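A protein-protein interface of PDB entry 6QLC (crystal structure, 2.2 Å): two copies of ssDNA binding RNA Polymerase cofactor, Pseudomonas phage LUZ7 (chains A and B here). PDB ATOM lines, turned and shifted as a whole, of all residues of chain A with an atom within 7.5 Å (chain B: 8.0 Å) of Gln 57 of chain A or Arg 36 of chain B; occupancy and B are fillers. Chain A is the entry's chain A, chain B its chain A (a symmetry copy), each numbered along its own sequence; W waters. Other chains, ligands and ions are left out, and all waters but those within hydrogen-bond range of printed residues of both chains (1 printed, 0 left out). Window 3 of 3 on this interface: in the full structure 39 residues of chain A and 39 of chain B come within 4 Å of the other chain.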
ATOM      1  N   LEU A  48       5.520 -12.231   4.093  1.00  0.00           N
ATOM      2  CA  LEU A  48       4.807 -13.066   5.059  1.00  0.00           C
ATOM      3  C   LEU A  48       3.314 -12.987   4.747  1.00  0.00           C
ATOM      4  O   LEU A  48       2.637 -12.021   5.116  1.00  0.00           O
ATOM      5  CB  LEU A  48       5.110 -12.631   6.490  1.00  0.00           C
ATOM      6  CG  LEU A  48       6.594 -12.372   6.792  1.00  0.00           C
ATOM      7  CD1 LEU A  48       6.763 -11.857   8.207  1.00  0.00           C
ATOM      8  CD2 LEU A  48       7.397 -13.632   6.592  1.00  0.00           C
ATOM      9  N   ARG A  49       2.810 -14.008   4.060  1.00  0.00           N
ATOM     10  CA  ARG A  49       1.403 -14.093   3.696  1.00  0.00           C
ATOM     11  C   ARG A  49       0.555 -14.457   4.913  1.00  0.00           C
ATOM     12  O   ARG A  49       0.894 -15.381   5.663  1.00  0.00           O
ATOM     13  CB  ARG A  49       1.223 -15.129   2.586  1.00  0.00           C
ATOM     14  CG  ARG A  49       2.162 -14.931   1.405  1.00  0.00           C
ATOM     15  CD  ARG A  49       2.206 -16.152   0.506  1.00  0.00           C
ATOM     16  NE  ARG A  49       0.872 -16.571   0.086  1.00  0.00           N
ATOM     17  CZ  ARG A  49       0.268 -16.150  -1.020  1.00  0.00           C
ATOM     18  NH1 ARG A  49       0.878 -15.293  -1.828  1.00  0.00           N
ATOM     19  NH2 ARG A  49      -0.948 -16.587  -1.319  1.00  0.00           N
ATOM     20  N   ASP A  52      -0.420 -18.089   5.653  1.00  0.00           N
ATOM     21  CA  ASP A  52       0.656 -19.052   5.877  1.00  0.00           C
ATOM     22  C   ASP A  52       0.995 -19.086   7.362  1.00  0.00           C
ATOM     23  O   ASP A  52       1.565 -18.128   7.900  1.00  0.00           O
ATOM     24  CB  ASP A  52       1.886 -18.697   5.045  1.00  0.00           C
ATOM     25  CG  ASP A  52       2.919 -19.804   5.033  1.00  0.00           C
ATOM     26  OD1 ASP A  52       3.191 -20.398   6.098  1.00  0.00           O
ATOM     27  OD2 ASP A  52       3.474 -20.071   3.949  1.00  0.00           O
ATOM     28  N   ALA A  53       0.673 -20.211   8.008  1.00  0.00           N
ATOM     29  CA  ALA A  53       0.890 -20.355   9.444  1.00  0.00           C
ATOM     30  C   ALA A  53       2.361 -20.266   9.823  1.00  0.00           C
ATOM     31  O   ALA A  53       2.683 -19.878  10.950  1.00  0.00           O
ATOM     32  CB  ALA A  53       0.323 -21.686   9.923  1.00  0.00           C
ATOM     33  N   LEU A  54       3.267 -20.673   8.931  1.00  0.00           N
ATOM     34  CA  LEU A  54       4.688 -20.443   9.185  1.00  0.00           C
ATOM     35  C   LEU A  54       4.985 -18.950   9.236  1.00  0.00           C
ATOM     36  O   LEU A  54       5.597 -18.457  10.193  1.00  0.00           O
ATOM     37  CB  LEU A  54       5.537 -21.112   8.105  1.00  0.00           C
ATOM     38  CG  LEU A  54       5.771 -22.615   8.238  1.00  0.00           C
ATOM     39  CD1 LEU A  54       7.086 -22.959   7.574  1.00  0.00           C
ATOM     40  CD2 LEU A  54       5.779 -23.038   9.690  1.00  0.00           C
ATOM     41  N   HIS A  55       4.542 -18.217   8.213  1.00  0.00           N
ATOM     42  CA  HIS A  55       4.811 -16.785   8.143  1.00  0.00           C
ATOM     43  C   HIS A  55       4.272 -16.067   9.367  1.00  0.00           C
ATOM     44  O   HIS A  55       4.967 -15.230   9.960  1.00  0.00           O
ATOM     45  CB  HIS A  55       4.209 -16.207   6.869  1.00  0.00           C
ATOM     46  CG  HIS A  55       4.814 -16.759   5.620  1.00  0.00           C
ATOM     47  ND1 HIS A  55       4.437 -16.345   4.361  1.00  0.00           N
ATOM     48  CD2 HIS A  55       5.775 -17.693   5.433  1.00  0.00           C
ATOM     49  CE1 HIS A  55       5.141 -16.993   3.452  1.00  0.00           C
ATOM     50  NE2 HIS A  55       5.963 -17.817   4.076  1.00  0.00           N
ATOM     51  N   MET A  56       3.054 -16.418   9.790  1.00  0.00           N
ATOM     52  CA  MET A  56       2.443 -15.728  10.916  1.00  0.00           C
ATOM     53  C   MET A  56       3.109 -16.110  12.225  1.00  0.00           C
ATOM     54  O   MET A  56       3.221 -15.284  13.136  1.00  0.00           O
ATOM     55  CB  MET A  56       0.943 -16.037  10.973  1.00  0.00           C
ATOM     56  CG  MET A  56       0.212 -15.784   9.665  1.00  0.00           C
ATOM     57  SD  MET A  56       0.621 -14.169   8.991  1.00  0.00           S
ATOM     58  CE  MET A  56      -0.077 -13.128  10.251  1.00  0.00           C
ATOM     59  N   GLN A  57       3.526 -17.367  12.356  1.00  0.00           N
ATOM     60  CA  GLN A  57       4.368 -17.731  13.492  1.00  0.00           C
ATOM     61  C   GLN A  57       5.657 -16.905  13.512  1.00  0.00           C
ATOM     62  O   GLN A  57       6.158 -16.538  14.583  1.00  0.00           O
ATOM     63  CB  GLN A  57       4.689 -19.222  13.433  1.00  0.00           C
ATOM     64  CG  GLN A  57       5.499 -19.731  14.605  1.00  0.00           C
ATOM     65  CD  GLN A  57       5.966 -21.152  14.407  1.00  0.00           C
ATOM     66  OE1 GLN A  57       5.840 -21.715  13.310  1.00  0.00           O
ATOM     67  NE2 GLN A  57       6.512 -21.747  15.464  1.00  0.00           N
ATOM     68  N   LEU A  58       6.215 -16.617  12.332  1.00  0.00           N
ATOM     69  CA  LEU A  58       7.427 -15.802  12.253  1.00  0.00           C
ATOM     70  C   LEU A  58       7.118 -14.360  12.614  1.00  0.00           C
ATOM     71  O   LEU A  58       7.805 -13.758  13.448  1.00  0.00           O
ATOM     72  CB  LEU A  58       8.023 -15.866  10.849  1.00  0.00           C
ATOM     73  CG  LEU A  58       9.111 -16.894  10.557  1.00  0.00           C
ATOM     74  CD1 LEU A  58       9.409 -16.898   9.073  1.00  0.00           C
ATOM     75  CD2 LEU A  58      10.357 -16.588  11.349  1.00  0.00           C
ATOM     76  N   GLN A  59       6.073 -13.801  11.993  1.00  0.00           N
ATOM     77  CA  GLN A  59       5.614 -12.453  12.314  1.00  0.00           C
ATOM     78  C   GLN A  59       5.369 -12.280  13.811  1.00  0.00           C
ATOM     79  O   GLN A  59       5.862 -11.329  14.424  1.00  0.00           O
ATOM     80  CB  GLN A  59       4.352 -12.151  11.512  1.00  0.00           C
ATOM     81  CG  GLN A  59       3.989 -10.689  11.408  1.00  0.00           C
ATOM     82  CD  GLN A  59       2.826 -10.453  10.455  1.00  0.00           C
ATOM     83  OE1 GLN A  59       3.014 -10.269   9.244  1.00  0.00           O
ATOM     84  NE2 GLN A  59       1.615 -10.470  10.999  1.00  0.00           N
ATOM     85  N   GLU A  60       4.623 -13.198  14.425  1.00  0.00           N
ATOM     86  CA  GLU A  60       4.362 -13.074  15.857  1.00  0.00           C
ATOM     87  C   GLU A  60       5.659 -13.096  16.648  1.00  0.00           C
ATOM     88  O   GLU A  60       5.832 -12.337  17.610  1.00  0.00           O
ATOM     89  CB  GLU A  60       3.457 -14.212  16.337  1.00  0.00           C
ATOM     90  CG  GLU A  60       1.990 -13.865  16.431  1.00  0.00           C
ATOM     91  CD  GLU A  60       1.171 -15.038  16.940  1.00  0.00           C
ATOM     92  OE1 GLU A  60       0.464 -15.671  16.121  1.00  0.00           O
ATOM     93  OE2 GLU A  60       1.255 -15.334  18.156  1.00  0.00           O
ATOM     94  N   PHE A  61       6.560 -13.998  16.279  1.00  0.00           N
ATOM     95  CA  PHE A  61       7.810 -14.149  17.001  1.00  0.00           C
ATOM     96  C   PHE A  61       8.617 -12.860  16.988  1.00  0.00           C
ATOM     97  O   PHE A  61       9.280 -12.532  17.976  1.00  0.00           O
ATOM     98  CB  PHE A  61       8.597 -15.287  16.373  1.00  0.00           C
ATOM     99  CG  PHE A  61       9.874 -15.575  17.053  1.00  0.00           C
ATOM    100  CD1 PHE A  61       9.882 -16.143  18.309  1.00  0.00           C
ATOM    101  CD2 PHE A  61      11.078 -15.278  16.431  1.00  0.00           C
ATOM    102  CE1 PHE A  61      11.070 -16.428  18.942  1.00  0.00           C
ATOM    103  CE2 PHE A  61      12.277 -15.550  17.059  1.00  0.00           C
ATOM    104  CZ  PHE A  61      12.273 -16.130  18.315  1.00  0.00           C
ATOM    105  N   LEU A  62       8.530 -12.099  15.901  1.00  0.00           N
ATOM    106  CA  LEU A  62       9.334 -10.900  15.712  1.00  0.00           C
ATOM    107  C   LEU A  62       8.593  -9.616  16.063  1.00  0.00           C
ATOM    108  O   LEU A  62       9.087  -8.530  15.749  1.00  0.00           O
ATOM    109  CB  LEU A  62       9.825 -10.826  14.269  1.00  0.00           C
ATOM    110  CG  LEU A  62      10.772 -11.950  13.876  1.00  0.00           C
ATOM    111  CD1 LEU A  62      11.501 -11.570  12.606  1.00  0.00           C
ATOM    112  CD2 LEU A  62      11.746 -12.195  15.018  1.00  0.00           C
ATOM    113  N   THR A  63       7.420  -9.711  16.697  1.00  0.00           N
ATOM    114  CA  THR A  63       6.618  -8.529  17.021  1.00  0.00           C
ATOM    115  C   THR A  63       6.075  -8.515  18.441  1.00  0.00           C
ATOM    116  O   THR A  63       5.836  -7.425  18.973  1.00  0.00           O
ATOM    117  CB  THR A  63       5.424  -8.405  16.070  1.00  0.00           C
ATOM    118  OG1 THR A  63       4.676  -9.621  16.113  1.00  0.00           O
ATOM    119  CG2 THR A  63       5.871  -8.155  14.654  1.00  0.00           C
ATOM    120  N   ARG A  79      15.802 -11.708  19.238  1.00  0.00           N
ATOM    121  CA  ARG A  79      15.100 -12.780  18.536  1.00  0.00           C
ATOM    122  C   ARG A  79      15.554 -12.883  17.087  1.00  0.00           C
ATOM    123  O   ARG A  79      15.705 -13.991  16.559  1.00  0.00           O
ATOM    124  CB  ARG A  79      13.586 -12.559  18.606  1.00  0.00           C
ATOM    125  CG  ARG A  79      12.990 -12.782  19.997  1.00  0.00           C
ATOM    126  CD  ARG A  79      11.454 -12.977  19.951  1.00  0.00           C
ATOM    127  NE  ARG A  79      10.936 -13.447  21.238  1.00  0.00           N
ATOM    128  CZ  ARG A  79       9.644 -13.495  21.561  1.00  0.00           C
ATOM    129  NH1 ARG A  79       8.710 -13.088  20.697  1.00  0.00           N
ATOM    130  NH2 ARG A  79       9.294 -13.932  22.764  1.00  0.00           N
ATOM    131  N   PHE B  33      15.065 -23.807   8.032  1.00  0.00           N
ATOM    132  CA  PHE B  33      14.930 -23.640   9.466  1.00  0.00           C
ATOM    133  C   PHE B  33      14.402 -24.911  10.126  1.00  0.00           C
ATOM    134  O   PHE B  33      13.531 -25.578   9.559  1.00  0.00           O
ATOM    135  CB  PHE B  33      13.999 -22.476   9.776  1.00  0.00           C
ATOM    136  CG  PHE B  33      14.148 -21.970  11.164  1.00  0.00           C
ATOM    137  CD1 PHE B  33      15.158 -21.060  11.481  1.00  0.00           C
ATOM    138  CD2 PHE B  33      13.307 -22.427  12.174  1.00  0.00           C
ATOM    139  CE1 PHE B  33      15.313 -20.596  12.790  1.00  0.00           C
ATOM    140  CE2 PHE B  33      13.444 -21.979  13.477  1.00  0.00           C
ATOM    141  CZ  PHE B  33      14.450 -21.058  13.795  1.00  0.00           C
ATOM    142  N   PRO B  34      14.914 -25.274  11.312  1.00  0.00           N
ATOM    143  CA  PRO B  34      14.433 -26.489  11.989  1.00  0.00           C
ATOM    144  C   PRO B  34      12.983 -26.363  12.438  1.00  0.00           C
ATOM    145  O   PRO B  34      12.545 -25.304  12.901  1.00  0.00           O
ATOM    146  CB  PRO B  34      15.375 -26.619  13.194  1.00  0.00           C
ATOM    147  CG  PRO B  34      15.865 -25.214  13.436  1.00  0.00           C
ATOM    148  CD  PRO B  34      16.023 -24.644  12.051  1.00  0.00           C
ATOM    149  N   THR B  35      12.243 -27.470  12.315  1.00  0.00           N
ATOM    150  CA  THR B  35      10.817 -27.560  12.645  1.00  0.00           C
ATOM    151  C   THR B  35      10.587 -28.478  13.848  1.00  0.00           C
ATOM    152  O   THR B  35      11.466 -29.235  14.258  1.00  0.00           O
ATOM    153  CB  THR B  35      10.004 -28.060  11.437  1.00  0.00           C
ATOM    154  OG1 THR B  35      10.602 -29.253  10.909  1.00  0.00           O
ATOM    155  CG2 THR B  35       9.998 -27.023  10.330  1.00  0.00           C
ATOM    156  N   ARG B  36       9.368 -28.424  14.405  1.00  0.00           N
ATOM    157  CA  ARG B  36       9.103 -29.101  15.677  1.00  0.00           C
ATOM    158  C   ARG B  36       9.149 -30.619  15.565  1.00  0.00           C
ATOM    159  O   ARG B  36       9.397 -31.285  16.572  1.00  0.00           O
ATOM    160  CB  ARG B  36       7.759 -28.673  16.247  1.00  0.00           C
ATOM    161  CG  ARG B  36       7.634 -27.173  16.460  1.00  0.00           C
ATOM    162  CD  ARG B  36       7.251 -26.819  17.895  1.00  0.00           C
ATOM    163  NE  ARG B  36       7.595 -25.432  18.210  1.00  0.00           N
ATOM    164  CZ  ARG B  36       6.747 -24.406  18.138  1.00  0.00           C
ATOM    165  NH1 ARG B  36       5.484 -24.603  17.769  1.00  0.00           N
ATOM    166  NH2 ARG B  36       7.165 -23.180  18.442  1.00  0.00           N
ATOM    167  N   ASP B  37       8.939 -31.174  14.375  1.00  0.00           N
ATOM    168  CA  ASP B  37       9.093 -32.600  14.130  1.00  0.00           C
ATOM    169  C   ASP B  37      10.542 -33.021  14.026  1.00  0.00           C
ATOM    170  O   ASP B  37      10.807 -34.153  13.612  1.00  0.00           O
ATOM    171  CB  ASP B  37       8.367 -32.996  12.842  1.00  0.00           C
ATOM    172  CG  ASP B  37       8.928 -32.281  11.609  1.00  0.00           C
ATOM    173  OD1 ASP B  37       9.921 -31.535  11.746  1.00  0.00           O
ATOM    174  OD2 ASP B  37       8.386 -32.467  10.504  1.00  0.00           O
ATOM    175  N   GLY B  38      11.486 -32.133  14.330  1.00  0.00           N
ATOM    176  CA  GLY B  38      12.880 -32.488  14.235  1.00  0.00           C
ATOM    177  C   GLY B  38      13.444 -32.533  12.835  1.00  0.00           C
ATOM    178  O   GLY B  38      14.619 -32.870  12.677  1.00  0.00           O
ATOM    179  N   LYS B  39      12.653 -32.227  11.804  1.00  0.00           N
ATOM    180  CA  LYS B  39      13.252 -32.039  10.481  1.00  0.00           C
ATOM    181  C   LYS B  39      13.491 -30.550  10.231  1.00  0.00           C
ATOM    182  O   LYS B  39      13.840 -29.818  11.161  1.00  0.00           O
ATOM    183  CB  LYS B  39      12.375 -32.637   9.385  1.00  0.00           C
ATOM    184  CG  LYS B  39      12.232 -34.153   9.458  1.00  0.00           C
ATOM    185  CD  LYS B  39      10.797 -34.574   9.172  1.00  0.00           C
ATOM    186  CE  LYS B  39      10.742 -35.946   8.518  1.00  0.00           C
ATOM    187  NZ  LYS B  39      11.471 -36.971   9.324  1.00  0.00           N
ATOM    188  N   ASP B  40      13.312 -30.081   8.996  1.00  0.00           N
ATOM    189  CA  ASP B  40      13.433 -28.657   8.731  1.00  0.00           C
ATOM    190  C   ASP B  40      12.417 -28.262   7.664  1.00  0.00           C
ATOM    191  O   ASP B  40      11.690 -29.104   7.125  1.00  0.00           O
ATOM    192  CB  ASP B  40      14.888 -28.282   8.368  1.00  0.00           C
ATOM    193  CG  ASP B  40      15.347 -28.814   7.010  1.00  0.00           C
ATOM    194  OD1 ASP B  40      14.524 -29.279   6.190  1.00  0.00           O
ATOM    195  OD2 ASP B  40      16.569 -28.735   6.749  1.00  0.00           O
ATOM    196  N   VAL B  41      12.351 -26.959   7.380  1.00  0.00           N
ATOM    197  CA  VAL B  41      11.503 -26.425   6.321  1.00  0.00           C
ATOM    198  C   VAL B  41      12.273 -25.330   5.579  1.00  0.00           C
ATOM    199  O   VAL B  41      13.000 -24.540   6.191  1.00  0.00           O
ATOM    200  CB  VAL B  41      10.166 -25.904   6.888  1.00  0.00           C
ATOM    201  CG1 VAL B  41      10.379 -24.706   7.805  1.00  0.00           C
ATOM    202  CG2 VAL B  41       9.179 -25.579   5.779  1.00  0.00           C
HETATM  203  O   HOH W   1       6.711 -19.900  17.832  1.00  0.00           O
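Hydrophobic or aromatic side chains of chain B within 4 Å of the printed part of chain A: Val 41. Hydrophobic or aromatic side chains of chain A that line the printed part of chain B: Leu 54. Among the printed residues, no Asp or Glu carboxylate lies within 4 Å of a Lys or Arg side-chain nitrogen of the other chain.
No position is printed for both chains.
The side-chain amide nitrogen (NE2) of Gln 57 of chain A sits close to the guanidinium group (NH2) of Arg 36 of chain B (3.4 Å).
Of the printed residues of chain A, Arg 36 of chain B touches Gln 57. Printed residues of chain B within 4 Å of Leu 54 of chain A: Val 41 (3.7 Å). Of the printed residues of chain A, Val 41 of chain B touches Leu 54 (3.7 Å). Leu 48 of chain A touches none of the printed residues of chain B. The nearest printed residue of chain A that does not touch Arg 36 of chain B is Phe 61 of chain A (7.5 Å).
N of Leu 54 of chain A lies within hydrogen-bond range of OD1 of Asp 52 of chain A (2.8 Å). O of Phe 33 of chain B sits at hydrogen-bond distance from N of Val 41 of chain B (2.8 Å).
Val 41 of chain B touches Leu 54 of chain A (CG1 to CD1, 3.7 Å).
Water W1 bridges the side-chain amide nitrogen (NE2) of Gln 57 of chain A and the guanidinium group (NH2) of Arg 36 of chain B.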
